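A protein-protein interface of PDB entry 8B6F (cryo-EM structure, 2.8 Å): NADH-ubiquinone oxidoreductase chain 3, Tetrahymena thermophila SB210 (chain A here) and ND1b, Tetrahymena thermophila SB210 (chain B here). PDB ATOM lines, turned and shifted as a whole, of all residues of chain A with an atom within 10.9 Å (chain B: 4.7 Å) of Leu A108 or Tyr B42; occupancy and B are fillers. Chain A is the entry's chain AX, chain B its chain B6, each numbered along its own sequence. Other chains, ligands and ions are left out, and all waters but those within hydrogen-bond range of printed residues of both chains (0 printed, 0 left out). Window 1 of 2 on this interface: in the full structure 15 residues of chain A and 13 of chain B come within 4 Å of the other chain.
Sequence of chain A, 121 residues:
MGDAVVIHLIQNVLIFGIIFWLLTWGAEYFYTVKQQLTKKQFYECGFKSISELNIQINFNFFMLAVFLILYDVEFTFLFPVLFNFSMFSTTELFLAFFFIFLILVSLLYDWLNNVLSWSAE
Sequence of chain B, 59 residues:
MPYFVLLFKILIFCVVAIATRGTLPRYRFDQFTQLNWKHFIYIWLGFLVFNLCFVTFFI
Among the printed residues, pairs that only touch across the chains: Leu A104 with Leu B45, Leu A107 with Ile B41, Tyr A71 with Trp B37, Leu A107 with Leu B45, Leu A116 with Trp B37, Trp A111 with Lys B38, Leu A64 with Trp B37 and Trp A111 with Tyr B42.
Hydrophobic or aromatic side chains of chain B that line the printed part of chain A: Trp B37, Ile B41, Tyr B42 and Leu B45. Along chain A the printed residues that touch a printed residue of chain B span positions 64 to 116. Among the printed residues, no Asp or Glu carboxylate lies within 4 Å of a Lys or Arg side-chain nitrogen of the other chain.
The side-chain hydroxyl (OH) of Tyr B42 is in hydrogen-bond range of the backbone carbonyl oxygen (O) of Leu A107 (2.8 Å). N of Leu A108 lies within hydrogen-bond range of OH of Tyr B42 (3.3 Å).
The backbone carbonyl oxygen (O) of Trp A111 sits at hydrogen-bond distance from the side-chain amide nitrogen (ND2) of Asn A114, 2.9 Å away.
Leu A102 touches none of the printed residues of chain B. Of the printed residues of chain B, Leu A104 touches Leu B45 (3.3 Å). Printed residues of chain B within 4 Å of Leu A108: Tyr B42 (3.3 Å). Of the printed residues of chain B, Trp A111 touches Lys B38 (3.8 Å) and Tyr B42 (3.96 Å). Of the printed residues of chain A, Trp B37 touches Leu A64 (3.9 Å), Tyr A71 (3.4 Å) and Leu A116 (3.8 Å). Ile B41 touches one residue of chain A. Of chain A, only Leu A107, Leu A108 and Trp A111 come within 4 Å of Tyr B42. No residue of chain A comes within 4 Å of Ile B43. Of the printed residues of chain A, Leu B45 touches Leu A104 and Leu A107. The nearest residue of chain A that does not touch Tyr B42 is Leu A104 (4.1 Å).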
ATOM      1  N   LEU A  64      -2.677 -11.607  -2.575  1.00  0.00           N
ATOM      2  CA  LEU A  64      -4.023 -12.068  -2.886  1.00  0.00           C
ATOM      3  C   LEU A  64      -4.723 -11.112  -3.842  1.00  0.00           C
ATOM      4  O   LEU A  64      -5.380 -11.546  -4.796  1.00  0.00           O
ATOM      5  CB  LEU A  64      -4.816 -12.223  -1.596  1.00  0.00           C
ATOM      6  CG  LEU A  64      -4.232 -13.268  -0.647  1.00  0.00           C
ATOM      7  CD1 LEU A  64      -4.929 -13.136   0.666  1.00  0.00           C
ATOM      8  CD2 LEU A  64      -4.383 -14.677  -1.197  1.00  0.00           C
ATOM      9  N   PHE A  67      -3.109 -11.436  -7.317  1.00  0.00           N
ATOM     10  CA  PHE A  67      -3.581 -12.601  -8.053  1.00  0.00           C
ATOM     11  C   PHE A  67      -5.050 -12.477  -8.421  1.00  0.00           C
ATOM     12  O   PHE A  67      -5.477 -13.018  -9.446  1.00  0.00           O
ATOM     13  CB  PHE A  67      -3.339 -13.867  -7.232  1.00  0.00           C
ATOM     14  CG  PHE A  67      -1.885 -14.177  -7.014  1.00  0.00           C
ATOM     15  CD1 PHE A  67      -0.964 -14.014  -8.036  1.00  0.00           C
ATOM     16  CD2 PHE A  67      -1.441 -14.626  -5.785  1.00  0.00           C
ATOM     17  CE1 PHE A  67       0.370 -14.296  -7.835  1.00  0.00           C
ATOM     18  CE2 PHE A  67      -0.111 -14.908  -5.579  1.00  0.00           C
ATOM     19  CZ  PHE A  67       0.798 -14.744  -6.606  1.00  0.00           C
ATOM     20  N   TYR A  71      -6.794 -13.243 -12.039  1.00  0.00           N
ATOM     21  CA  TYR A  71      -7.765 -14.325 -12.157  1.00  0.00           C
ATOM     22  C   TYR A  71      -9.151 -13.812 -12.517  1.00  0.00           C
ATOM     23  O   TYR A  71      -9.945 -14.555 -13.104  1.00  0.00           O
ATOM     24  CB  TYR A  71      -7.804 -15.132 -10.861  1.00  0.00           C
ATOM     25  CG  TYR A  71      -6.481 -15.781 -10.519  1.00  0.00           C
ATOM     26  CD1 TYR A  71      -5.550 -16.081 -11.508  1.00  0.00           C
ATOM     27  CD2 TYR A  71      -6.156 -16.085  -9.208  1.00  0.00           C
ATOM     28  CE1 TYR A  71      -4.342 -16.668 -11.200  1.00  0.00           C
ATOM     29  CE2 TYR A  71      -4.947 -16.673  -8.891  1.00  0.00           C
ATOM     30  CZ  TYR A  71      -4.045 -16.961  -9.892  1.00  0.00           C
ATOM     31  OH  TYR A  71      -2.841 -17.545  -9.580  1.00  0.00           O
ATOM     32  N   GLU A  74      -8.902 -13.781 -16.171  1.00  0.00           N
ATOM     33  CA  GLU A  74      -8.867 -15.159 -16.646  1.00  0.00           C
ATOM     34  C   GLU A  74     -10.262 -15.763 -16.653  1.00  0.00           C
ATOM     35  O   GLU A  74     -10.656 -16.424 -17.620  1.00  0.00           O
ATOM     36  CB  GLU A  74      -7.922 -15.990 -15.780  1.00  0.00           C
ATOM     37  CG  GLU A  74      -6.455 -15.656 -15.987  1.00  0.00           C
ATOM     38  CD  GLU A  74      -5.528 -16.522 -15.157  1.00  0.00           C
ATOM     39  OE1 GLU A  74      -6.018 -17.211 -14.239  1.00  0.00           O
ATOM     40  OE2 GLU A  74      -4.308 -16.519 -15.424  1.00  0.00           O
ATOM     41  N   PHE A  75     -11.024 -15.547 -15.583  1.00  0.00           N
ATOM     42  CA  PHE A  75     -12.392 -16.048 -15.540  1.00  0.00           C
ATOM     43  C   PHE A  75     -13.273 -15.327 -16.552  1.00  0.00           C
ATOM     44  O   PHE A  75     -14.127 -15.951 -17.194  1.00  0.00           O
ATOM     45  CB  PHE A  75     -12.958 -15.895 -14.128  1.00  0.00           C
ATOM     46  CG  PHE A  75     -12.170 -16.625 -13.074  1.00  0.00           C
ATOM     47  CD1 PHE A  75     -11.402 -17.734 -13.396  1.00  0.00           C
ATOM     48  CD2 PHE A  75     -12.201 -16.200 -11.755  1.00  0.00           C
ATOM     49  CE1 PHE A  75     -10.681 -18.401 -12.426  1.00  0.00           C
ATOM     50  CE2 PHE A  75     -11.482 -16.862 -10.781  1.00  0.00           C
ATOM     51  CZ  PHE A  75     -10.720 -17.966 -11.117  1.00  0.00           C
ATOM     52  N   ILE A 100      -8.120 -23.384 -19.036  1.00  0.00           N
ATOM     53  CA  ILE A 100      -8.411 -23.812 -17.670  1.00  0.00           C
ATOM     54  C   ILE A 100      -7.188 -24.473 -17.051  1.00  0.00           C
ATOM     55  O   ILE A 100      -6.889 -24.279 -15.868  1.00  0.00           O
ATOM     56  CB  ILE A 100      -9.637 -24.742 -17.646  1.00  0.00           C
ATOM     57  CG1 ILE A 100     -10.883 -23.983 -18.106  1.00  0.00           C
ATOM     58  CG2 ILE A 100      -9.852 -25.315 -16.248  1.00  0.00           C
ATOM     59  CD1 ILE A 100     -12.090 -24.864 -18.347  1.00  0.00           C
ATOM     60  N   PHE A 101      -6.458 -25.260 -17.841  1.00  0.00           N
ATOM     61  CA  PHE A 101      -5.246 -25.889 -17.334  1.00  0.00           C
ATOM     62  C   PHE A 101      -4.198 -24.845 -16.976  1.00  0.00           C
ATOM     63  O   PHE A 101      -3.501 -24.978 -15.965  1.00  0.00           O
ATOM     64  CB  PHE A 101      -4.693 -26.873 -18.361  1.00  0.00           C
ATOM     65  CG  PHE A 101      -3.528 -27.671 -17.861  1.00  0.00           C
ATOM     66  CD1 PHE A 101      -3.724 -28.804 -17.094  1.00  0.00           C
ATOM     67  CD2 PHE A 101      -2.238 -27.282 -18.150  1.00  0.00           C
ATOM     68  CE1 PHE A 101      -2.650 -29.536 -16.631  1.00  0.00           C
ATOM     69  CE2 PHE A 101      -1.159 -28.007 -17.690  1.00  0.00           C
ATOM     70  CZ  PHE A 101      -1.366 -29.137 -16.929  1.00  0.00           C
ATOM     71  N   LEU A 102      -4.073 -23.794 -17.788  1.00  0.00           N
ATOM     72  CA  LEU A 102      -3.142 -22.724 -17.454  1.00  0.00           C
ATOM     73  C   LEU A 102      -3.514 -22.070 -16.130  1.00  0.00           C
ATOM     74  O   LEU A 102      -2.640 -21.786 -15.303  1.00  0.00           O
ATOM     75  CB  LEU A 102      -3.109 -21.681 -18.568  1.00  0.00           C
ATOM     76  CG  LEU A 102      -2.435 -22.075 -19.882  1.00  0.00           C
ATOM     77  CD1 LEU A 102      -2.611 -20.957 -20.886  1.00  0.00           C
ATOM     78  CD2 LEU A 102      -0.962 -22.392 -19.687  1.00  0.00           C
ATOM     79  N   ILE A 103      -4.803 -21.814 -15.913  1.00  0.00           N
ATOM     80  CA  ILE A 103      -5.238 -21.223 -14.650  1.00  0.00           C
ATOM     81  C   ILE A 103      -4.880 -22.144 -13.492  1.00  0.00           C
ATOM     82  O   ILE A 103      -4.358 -21.704 -12.462  1.00  0.00           O
ATOM     83  CB  ILE A 103      -6.749 -20.926 -14.685  1.00  0.00           C
ATOM     84  CG1 ILE A 103      -7.068 -19.926 -15.797  1.00  0.00           C
ATOM     85  CG2 ILE A 103      -7.216 -20.392 -13.335  1.00  0.00           C
ATOM     86  CD1 ILE A 103      -8.548 -19.661 -15.990  1.00  0.00           C
ATOM     87  N   LEU A 104      -5.153 -23.440 -13.644  1.00  0.00           N
ATOM     88  CA  LEU A 104      -4.849 -24.388 -12.578  1.00  0.00           C
ATOM     89  C   LEU A 104      -3.358 -24.424 -12.278  1.00  0.00           C
ATOM     90  O   LEU A 104      -2.953 -24.494 -11.113  1.00  0.00           O
ATOM     91  CB  LEU A 104      -5.347 -25.782 -12.957  1.00  0.00           C
ATOM     92  CG  LEU A 104      -6.862 -25.992 -12.972  1.00  0.00           C
ATOM     93  CD1 LEU A 104      -7.194 -27.355 -13.550  1.00  0.00           C
ATOM     94  CD2 LEU A 104      -7.446 -25.849 -11.579  1.00  0.00           C
ATOM     95  N   VAL A 105      -2.525 -24.384 -13.318  1.00  0.00           N
ATOM     96  CA  VAL A 105      -1.082 -24.447 -13.107  1.00  0.00           C
ATOM     97  C   VAL A 105      -0.584 -23.190 -12.405  1.00  0.00           C
ATOM     98  O   VAL A 105       0.300 -23.256 -11.546  1.00  0.00           O
ATOM     99  CB  VAL A 105      -0.353 -24.674 -14.442  1.00  0.00           C
ATOM    100  CG1 VAL A 105       1.144 -24.529 -14.250  1.00  0.00           C
ATOM    101  CG2 VAL A 105      -0.677 -26.047 -14.994  1.00  0.00           C
ATOM    102  N   SER A 106      -1.130 -22.025 -12.761  1.00  0.00           N
ATOM    103  CA  SER A 106      -0.744 -20.804 -12.064  1.00  0.00           C
ATOM    104  C   SER A 106      -1.123 -20.878 -10.591  1.00  0.00           C
ATOM    105  O   SER A 106      -0.340 -20.485  -9.720  1.00  0.00           O
ATOM    106  CB  SER A 106      -1.391 -19.589 -12.729  1.00  0.00           C
ATOM    107  OG  SER A 106      -2.804 -19.665 -12.664  1.00  0.00           O
ATOM    108  N   LEU A 107      -2.327 -21.369 -10.292  1.00  0.00           N
ATOM    109  CA  LEU A 107      -2.729 -21.528  -8.900  1.00  0.00           C
ATOM    110  C   LEU A 107      -1.810 -22.501  -8.176  1.00  0.00           C
ATOM    111  O   LEU A 107      -1.439 -22.276  -7.019  1.00  0.00           O
ATOM    112  CB  LEU A 107      -4.179 -22.006  -8.824  1.00  0.00           C
ATOM    113  CG  LEU A 107      -5.242 -21.007  -9.273  1.00  0.00           C
ATOM    114  CD1 LEU A 107      -6.592 -21.689  -9.391  1.00  0.00           C
ATOM    115  CD2 LEU A 107      -5.314 -19.848  -8.301  1.00  0.00           C
ATOM    116  N   LEU A 108      -1.439 -23.598  -8.839  1.00  0.00           N
ATOM    117  CA  LEU A 108      -0.551 -24.577  -8.222  1.00  0.00           C
ATOM    118  C   LEU A 108       0.816 -23.974  -7.929  1.00  0.00           C
ATOM    119  O   LEU A 108       1.397 -24.223  -6.866  1.00  0.00           O
ATOM    120  CB  LEU A 108      -0.418 -25.803  -9.127  1.00  0.00           C
ATOM    121  CG  LEU A 108       0.527 -26.906  -8.641  1.00  0.00           C
ATOM    122  CD1 LEU A 108       0.090 -27.443  -7.289  1.00  0.00           C
ATOM    123  CD2 LEU A 108       0.601 -28.024  -9.663  1.00  0.00           C
ATOM    124  N   TYR A 109       1.343 -23.173  -8.855  1.00  0.00           N
ATOM    125  CA  TYR A 109       2.625 -22.517  -8.619  1.00  0.00           C
ATOM    126  C   TYR A 109       2.538 -21.554  -7.444  1.00  0.00           C
ATOM    127  O   TYR A 109       3.456 -21.484  -6.620  1.00  0.00           O
ATOM    128  CB  TYR A 109       3.083 -21.786  -9.879  1.00  0.00           C
ATOM    129  CG  TYR A 109       4.426 -21.112  -9.730  1.00  0.00           C
ATOM    130  CD1 TYR A 109       5.605 -21.822  -9.911  1.00  0.00           C
ATOM    131  CD2 TYR A 109       4.515 -19.765  -9.409  1.00  0.00           C
ATOM    132  CE1 TYR A 109       6.834 -21.211  -9.776  1.00  0.00           C
ATOM    133  CE2 TYR A 109       5.739 -19.144  -9.272  1.00  0.00           C
ATOM    134  CZ  TYR A 109       6.895 -19.872  -9.457  1.00  0.00           C
ATOM    135  OH  TYR A 109       8.117 -19.259  -9.321  1.00  0.00           O
ATOM    136  N   ASP A 110       1.444 -20.798  -7.350  1.00  0.00           N
ATOM    137  CA  ASP A 110       1.262 -19.910  -6.208  1.00  0.00           C
ATOM    138  C   ASP A 110       1.261 -20.698  -4.904  1.00  0.00           C
ATOM    139  O   ASP A 110       1.903 -20.297  -3.927  1.00  0.00           O
ATOM    140  CB  ASP A 110      -0.039 -19.122  -6.360  1.00  0.00           C
ATOM    141  CG  ASP A 110      -0.057 -18.264  -7.609  1.00  0.00           C
ATOM    142  OD1 ASP A 110       1.028 -17.826  -8.045  1.00  0.00           O
ATOM    143  OD2 ASP A 110      -1.153 -18.024  -8.155  1.00  0.00           O
ATOM    144  N   TRP A 111       0.545 -21.823  -4.869  1.00  0.00           N
ATOM    145  CA  TRP A 111       0.533 -22.655  -3.670  1.00  0.00           C
ATOM    146  C   TRP A 111       1.927 -23.171  -3.342  1.00  0.00           C
ATOM    147  O   TRP A 111       2.343 -23.161  -2.178  1.00  0.00           O
ATOM    148  CB  TRP A 111      -0.441 -23.821  -3.834  1.00  0.00           C
ATOM    149  CG  TRP A 111      -0.523 -24.666  -2.603  1.00  0.00           C
ATOM    150  CD1 TRP A 111      -1.429 -24.549  -1.594  1.00  0.00           C
ATOM    151  CD2 TRP A 111       0.339 -25.755  -2.246  1.00  0.00           C
ATOM    152  NE1 TRP A 111      -1.186 -25.493  -0.628  1.00  0.00           N
ATOM    153  CE2 TRP A 111      -0.103 -26.245  -1.003  1.00  0.00           C
ATOM    154  CE3 TRP A 111       1.444 -26.359  -2.854  1.00  0.00           C
ATOM    155  CZ2 TRP A 111       0.508 -27.320  -0.363  1.00  0.00           C
ATOM    156  CZ3 TRP A 111       2.057 -27.424  -2.211  1.00  0.00           C
ATOM    157  CH2 TRP A 111       1.587 -27.893  -0.979  1.00  0.00           C
ATOM    158  N   LEU A 112       2.668 -23.621  -4.354  1.00  0.00           N
ATOM    159  CA  LEU A 112       4.008 -24.147  -4.112  1.00  0.00           C
ATOM    160  C   LEU A 112       4.910 -23.091  -3.488  1.00  0.00           C
ATOM    161  O   LEU A 112       5.672 -23.386  -2.561  1.00  0.00           O
ATOM    162  CB  LEU A 112       4.617 -24.652  -5.421  1.00  0.00           C
ATOM    163  CG  LEU A 112       4.030 -25.929  -6.023  1.00  0.00           C
ATOM    164  CD1 LEU A 112       4.606 -26.174  -7.406  1.00  0.00           C
ATOM    165  CD2 LEU A 112       4.295 -27.120  -5.127  1.00  0.00           C
ATOM    166  N   ASN A 113       4.843 -21.859  -3.982  1.00  0.00           N
ATOM    167  CA  ASN A 113       5.679 -20.789  -3.455  1.00  0.00           C
ATOM    168  C   ASN A 113       5.137 -20.185  -2.165  1.00  0.00           C
ATOM    169  O   ASN A 113       5.842 -19.394  -1.531  1.00  0.00           O
ATOM    170  CB  ASN A 113       5.843 -19.696  -4.508  1.00  0.00           C
ATOM    171  CG  ASN A 113       6.917 -20.030  -5.515  1.00  0.00           C
ATOM    172  OD1 ASN A 113       8.047 -19.556  -5.416  1.00  0.00           O
ATOM    173  ND2 ASN A 113       6.573 -20.864  -6.488  1.00  0.00           N
ATOM    174  N   ASN A 114       3.917 -20.533  -1.761  1.00  0.00           N
ATOM    175  CA  ASN A 114       3.372 -20.124  -0.467  1.00  0.00           C
ATOM    176  C   ASN A 114       3.226 -18.607  -0.385  1.00  0.00           C
ATOM    177  O   ASN A 114       3.623 -17.971   0.592  1.00  0.00           O
ATOM    178  CB  ASN A 114       4.232 -20.650   0.684  1.00  0.00           C
ATOM    179  CG  ASN A 114       4.372 -22.157   0.663  1.00  0.00           C
ATOM    180  OD1 ASN A 114       5.479 -22.690   0.716  1.00  0.00           O
ATOM    181  ND2 ASN A 114       3.244 -22.855   0.581  1.00  0.00           N
ATOM    182  N   VAL A 115       2.645 -18.026  -1.436  1.00  0.00           N
ATOM    183  CA  VAL A 115       2.373 -16.595  -1.475  1.00  0.00           C
ATOM    184  C   VAL A 115       0.917 -16.281  -1.174  1.00  0.00           C
ATOM    185  O   VAL A 115       0.512 -15.114  -1.255  1.00  0.00           O
ATOM    186  CB  VAL A 115       2.772 -15.989  -2.838  1.00  0.00           C
ATOM    187  CG1 VAL A 115       4.282 -15.973  -2.986  1.00  0.00           C
ATOM    188  CG2 VAL A 115       2.138 -16.768  -3.983  1.00  0.00           C
ATOM    189  N   LEU A 116       0.117 -17.288  -0.820  1.00  0.00           N
ATOM    190  CA  LEU A 116      -1.301 -17.121  -0.533  1.00  0.00           C
ATOM    191  C   LEU A 116      -1.581 -17.054   0.964  1.00  0.00           C
ATOM    192  O   LEU A 116      -2.674 -17.421   1.407  1.00  0.00           O
ATOM    193  CB  LEU A 116      -2.101 -18.258  -1.169  1.00  0.00           C
ATOM    194  CG  LEU A 116      -1.905 -18.472  -2.672  1.00  0.00           C
ATOM    195  CD1 LEU A 116      -2.656 -19.706  -3.137  1.00  0.00           C
ATOM    196  CD2 LEU A 116      -2.355 -17.249  -3.456  1.00  0.00           C
ATOM    197  N   TRP B  37      -8.521 -20.034  -1.334  1.00  0.00           N
ATOM    198  CA  TRP B  37      -7.536 -20.006  -2.405  1.00  0.00           C
ATOM    199  C   TRP B  37      -6.698 -21.275  -2.499  1.00  0.00           C
ATOM    200  O   TRP B  37      -5.991 -21.445  -3.496  1.00  0.00           O
ATOM    201  CB  TRP B  37      -6.610 -18.803  -2.221  1.00  0.00           C
ATOM    202  CG  TRP B  37      -7.273 -17.495  -2.494  1.00  0.00           C
ATOM    203  CD1 TRP B  37      -8.112 -16.812  -1.664  1.00  0.00           C
ATOM    204  CD2 TRP B  37      -7.153 -16.708  -3.682  1.00  0.00           C
ATOM    205  NE1 TRP B  37      -8.521 -15.646  -2.263  1.00  0.00           N
ATOM    206  CE2 TRP B  37      -7.944 -15.557  -3.502  1.00  0.00           C
ATOM    207  CE3 TRP B  37      -6.449 -16.863  -4.879  1.00  0.00           C
ATOM    208  CZ2 TRP B  37      -8.056 -14.571  -4.478  1.00  0.00           C
ATOM    209  CZ3 TRP B  37      -6.559 -15.882  -5.847  1.00  0.00           C
ATOM    210  CH2 TRP B  37      -7.358 -14.749  -5.640  1.00  0.00           C
ATOM    211  N   LYS B  38      -6.751 -22.162  -1.505  1.00  0.00           N
ATOM    212  CA  LYS B  38      -5.991 -23.405  -1.565  1.00  0.00           C
ATOM    213  C   LYS B  38      -6.835 -24.622  -1.908  1.00  0.00           C
ATOM    214  O   LYS B  38      -6.310 -25.572  -2.497  1.00  0.00           O
ATOM    215  CB  LYS B  38      -5.284 -23.662  -0.231  1.00  0.00           C
ATOM    216  CG  LYS B  38      -4.231 -22.624   0.121  1.00  0.00           C
ATOM    217  CD  LYS B  38      -3.604 -22.918   1.473  1.00  0.00           C
ATOM    218  CE  LYS B  38      -2.637 -21.823   1.886  1.00  0.00           C
ATOM    219  NZ  LYS B  38      -1.495 -21.694   0.942  1.00  0.00           N
ATOM    220  N   HIS B  39      -8.118 -24.628  -1.555  1.00  0.00           N
ATOM    221  CA  HIS B  39      -8.967 -25.790  -1.775  1.00  0.00           C
ATOM    222  C   HIS B  39     -10.167 -25.486  -2.656  1.00  0.00           C
ATOM    223  O   HIS B  39     -10.422 -26.216  -3.619  1.00  0.00           O
ATOM    224  CB  HIS B  39      -9.438 -26.339  -0.416  1.00  0.00           C
ATOM    225  CG  HIS B  39     -10.222 -27.610  -0.514  1.00  0.00           C
ATOM    226  ND1 HIS B  39      -9.691 -28.775  -1.027  1.00  0.00           N
ATOM    227  CD2 HIS B  39     -11.496 -27.900  -0.162  1.00  0.00           C
ATOM    228  CE1 HIS B  39     -10.607 -29.726  -0.991  1.00  0.00           C
ATOM    229  NE2 HIS B  39     -11.711 -29.222  -0.468  1.00  0.00           N
ATOM    230  N   PHE B  40     -10.904 -24.414  -2.366  1.00  0.00           N
ATOM    231  CA  PHE B  40     -12.220 -24.239  -2.967  1.00  0.00           C
ATOM    232  C   PHE B  40     -12.143 -23.763  -4.408  1.00  0.00           C
ATOM    233  O   PHE B  40     -13.009 -24.112  -5.216  1.00  0.00           O
ATOM    234  CB  PHE B  40     -13.057 -23.269  -2.133  1.00  0.00           C
ATOM    235  CG  PHE B  40     -13.435 -23.805  -0.781  1.00  0.00           C
ATOM    236  CD1 PHE B  40     -13.821 -25.128  -0.629  1.00  0.00           C
ATOM    237  CD2 PHE B  40     -13.400 -22.991   0.336  1.00  0.00           C
ATOM    238  CE1 PHE B  40     -14.167 -25.624   0.610  1.00  0.00           C
ATOM    239  CE2 PHE B  40     -13.745 -23.484   1.580  1.00  0.00           C
ATOM    240  CZ  PHE B  40     -14.129 -24.802   1.715  1.00  0.00           C
ATOM    241  N   ILE B  41     -11.123 -22.979  -4.756  1.00  0.00           N
ATOM    242  CA  ILE B  41     -10.952 -22.586  -6.150  1.00  0.00           C
ATOM    243  C   ILE B  41     -10.693 -23.813  -7.015  1.00  0.00           C
ATOM    244  O   ILE B  41     -11.267 -23.957  -8.100  1.00  0.00           O
ATOM    245  CB  ILE B  41      -9.830 -21.535  -6.276  1.00  0.00           C
ATOM    246  CG1 ILE B  41      -9.755 -21.010  -7.711  1.00  0.00           C
ATOM    247  CG2 ILE B  41      -8.484 -22.113  -5.852  1.00  0.00           C
ATOM    248  CD1 ILE B  41      -8.873 -19.792  -7.877  1.00  0.00           C
ATOM    249  N   TYR B  42      -9.832 -24.718  -6.547  1.00  0.00           N
ATOM    250  CA  TYR B  42      -9.594 -25.954  -7.281  1.00  0.00           C
ATOM    251  C   TYR B  42     -10.859 -26.798  -7.365  1.00  0.00           C
ATOM    252  O   TYR B  42     -11.136 -27.413  -8.401  1.00  0.00           O
ATOM    253  CB  TYR B  42      -8.470 -26.748  -6.618  1.00  0.00           C
ATOM    254  CG  TYR B  42      -7.153 -26.013  -6.548  1.00  0.00           C
ATOM    255  CD1 TYR B  42      -6.282 -25.995  -7.629  1.00  0.00           C
ATOM    256  CD2 TYR B  42      -6.775 -25.349  -5.390  1.00  0.00           C
ATOM    257  CE1 TYR B  42      -5.072 -25.329  -7.559  1.00  0.00           C
ATOM    258  CE2 TYR B  42      -5.571 -24.680  -5.310  1.00  0.00           C
ATOM    259  CZ  TYR B  42      -4.725 -24.674  -6.397  1.00  0.00           C
ATOM    260  OH  TYR B  42      -3.526 -24.006  -6.311  1.00  0.00           O
ATOM    261  N   ILE B  43     -11.634 -26.852  -6.281  1.00  0.00           N
ATOM    262  CA  ILE B  43     -12.879 -27.617  -6.298  1.00  0.00           C
ATOM    263  C   ILE B  43     -13.829 -27.056  -7.348  1.00  0.00           C
ATOM    264  O   ILE B  43     -14.439 -27.804  -8.121  1.00  0.00           O
ATOM    265  CB  ILE B  43     -13.523 -27.624  -4.899  1.00  0.00           C
ATOM    266  CG1 ILE B  43     -12.675 -28.438  -3.914  1.00  0.00           C
ATOM    267  CG2 ILE B  43     -14.953 -28.163  -4.960  1.00  0.00           C
ATOM    268  CD1 ILE B  43     -12.702 -29.936  -4.132  1.00  0.00           C
ATOM    269  N   TRP B  44     -13.977 -25.730  -7.387  1.00  0.00           N
ATOM    270  CA  TRP B  44     -14.863 -25.118  -8.374  1.00  0.00           C
ATOM    271  C   TRP B  44     -14.397 -25.419  -9.791  1.00  0.00           C
ATOM    272  O   TRP B  44     -15.200 -25.782 -10.658  1.00  0.00           O
ATOM    273  CB  TRP B  44     -14.933 -23.609  -8.156  1.00  0.00           C
ATOM    274  CG  TRP B  44     -15.814 -23.170  -7.030  1.00  0.00           C
ATOM    275  CD1 TRP B  44     -15.432 -22.514  -5.896  1.00  0.00           C
ATOM    276  CD2 TRP B  44     -17.232 -23.346  -6.932  1.00  0.00           C
ATOM    277  NE1 TRP B  44     -16.523 -22.273  -5.099  1.00  0.00           N
ATOM    278  CE2 TRP B  44     -17.640 -22.774  -5.713  1.00  0.00           C
ATOM    279  CE3 TRP B  44     -18.194 -23.934  -7.758  1.00  0.00           C
ATOM    280  CZ2 TRP B  44     -18.969 -22.773  -5.299  1.00  0.00           C
ATOM    281  CZ3 TRP B  44     -19.514 -23.931  -7.345  1.00  0.00           C
ATOM    282  CH2 TRP B  44     -19.889 -23.355  -6.126  1.00  0.00           C
ATOM    283  N   LEU B  45     -13.097 -25.264 -10.049  1.00  0.00           N
ATOM    284  CA  LEU B  45     -12.583 -25.497 -11.394  1.00  0.00           C
ATOM    285  C   LEU B  45     -12.731 -26.957 -11.795  1.00  0.00           C
ATOM    286  O   LEU B  45     -13.113 -27.259 -12.928  1.00  0.00           O
ATOM    287  CB  LEU B  45     -11.123 -25.053 -11.488  1.00  0.00           C
ATOM    288  CG  LEU B  45     -10.893 -23.542 -11.371  1.00  0.00           C
ATOM    289  CD1 LEU B  45      -9.410 -23.226 -11.310  1.00  0.00           C
ATOM    290  CD2 LEU B  45     -11.541 -22.793 -12.526  1.00  0.00           C
ATOM    291  N   GLY B  46     -12.459 -27.878 -10.871  1.00  0.00           N
ATOM    292  CA  GLY B  46     -12.657 -29.285 -11.172  1.00  0.00           C
ATOM    293  C   GLY B  46     -14.110 -29.612 -11.455  1.00  0.00           C
ATOM    294  O   GLY B  46     -14.416 -30.383 -12.365  1.00  0.00           O
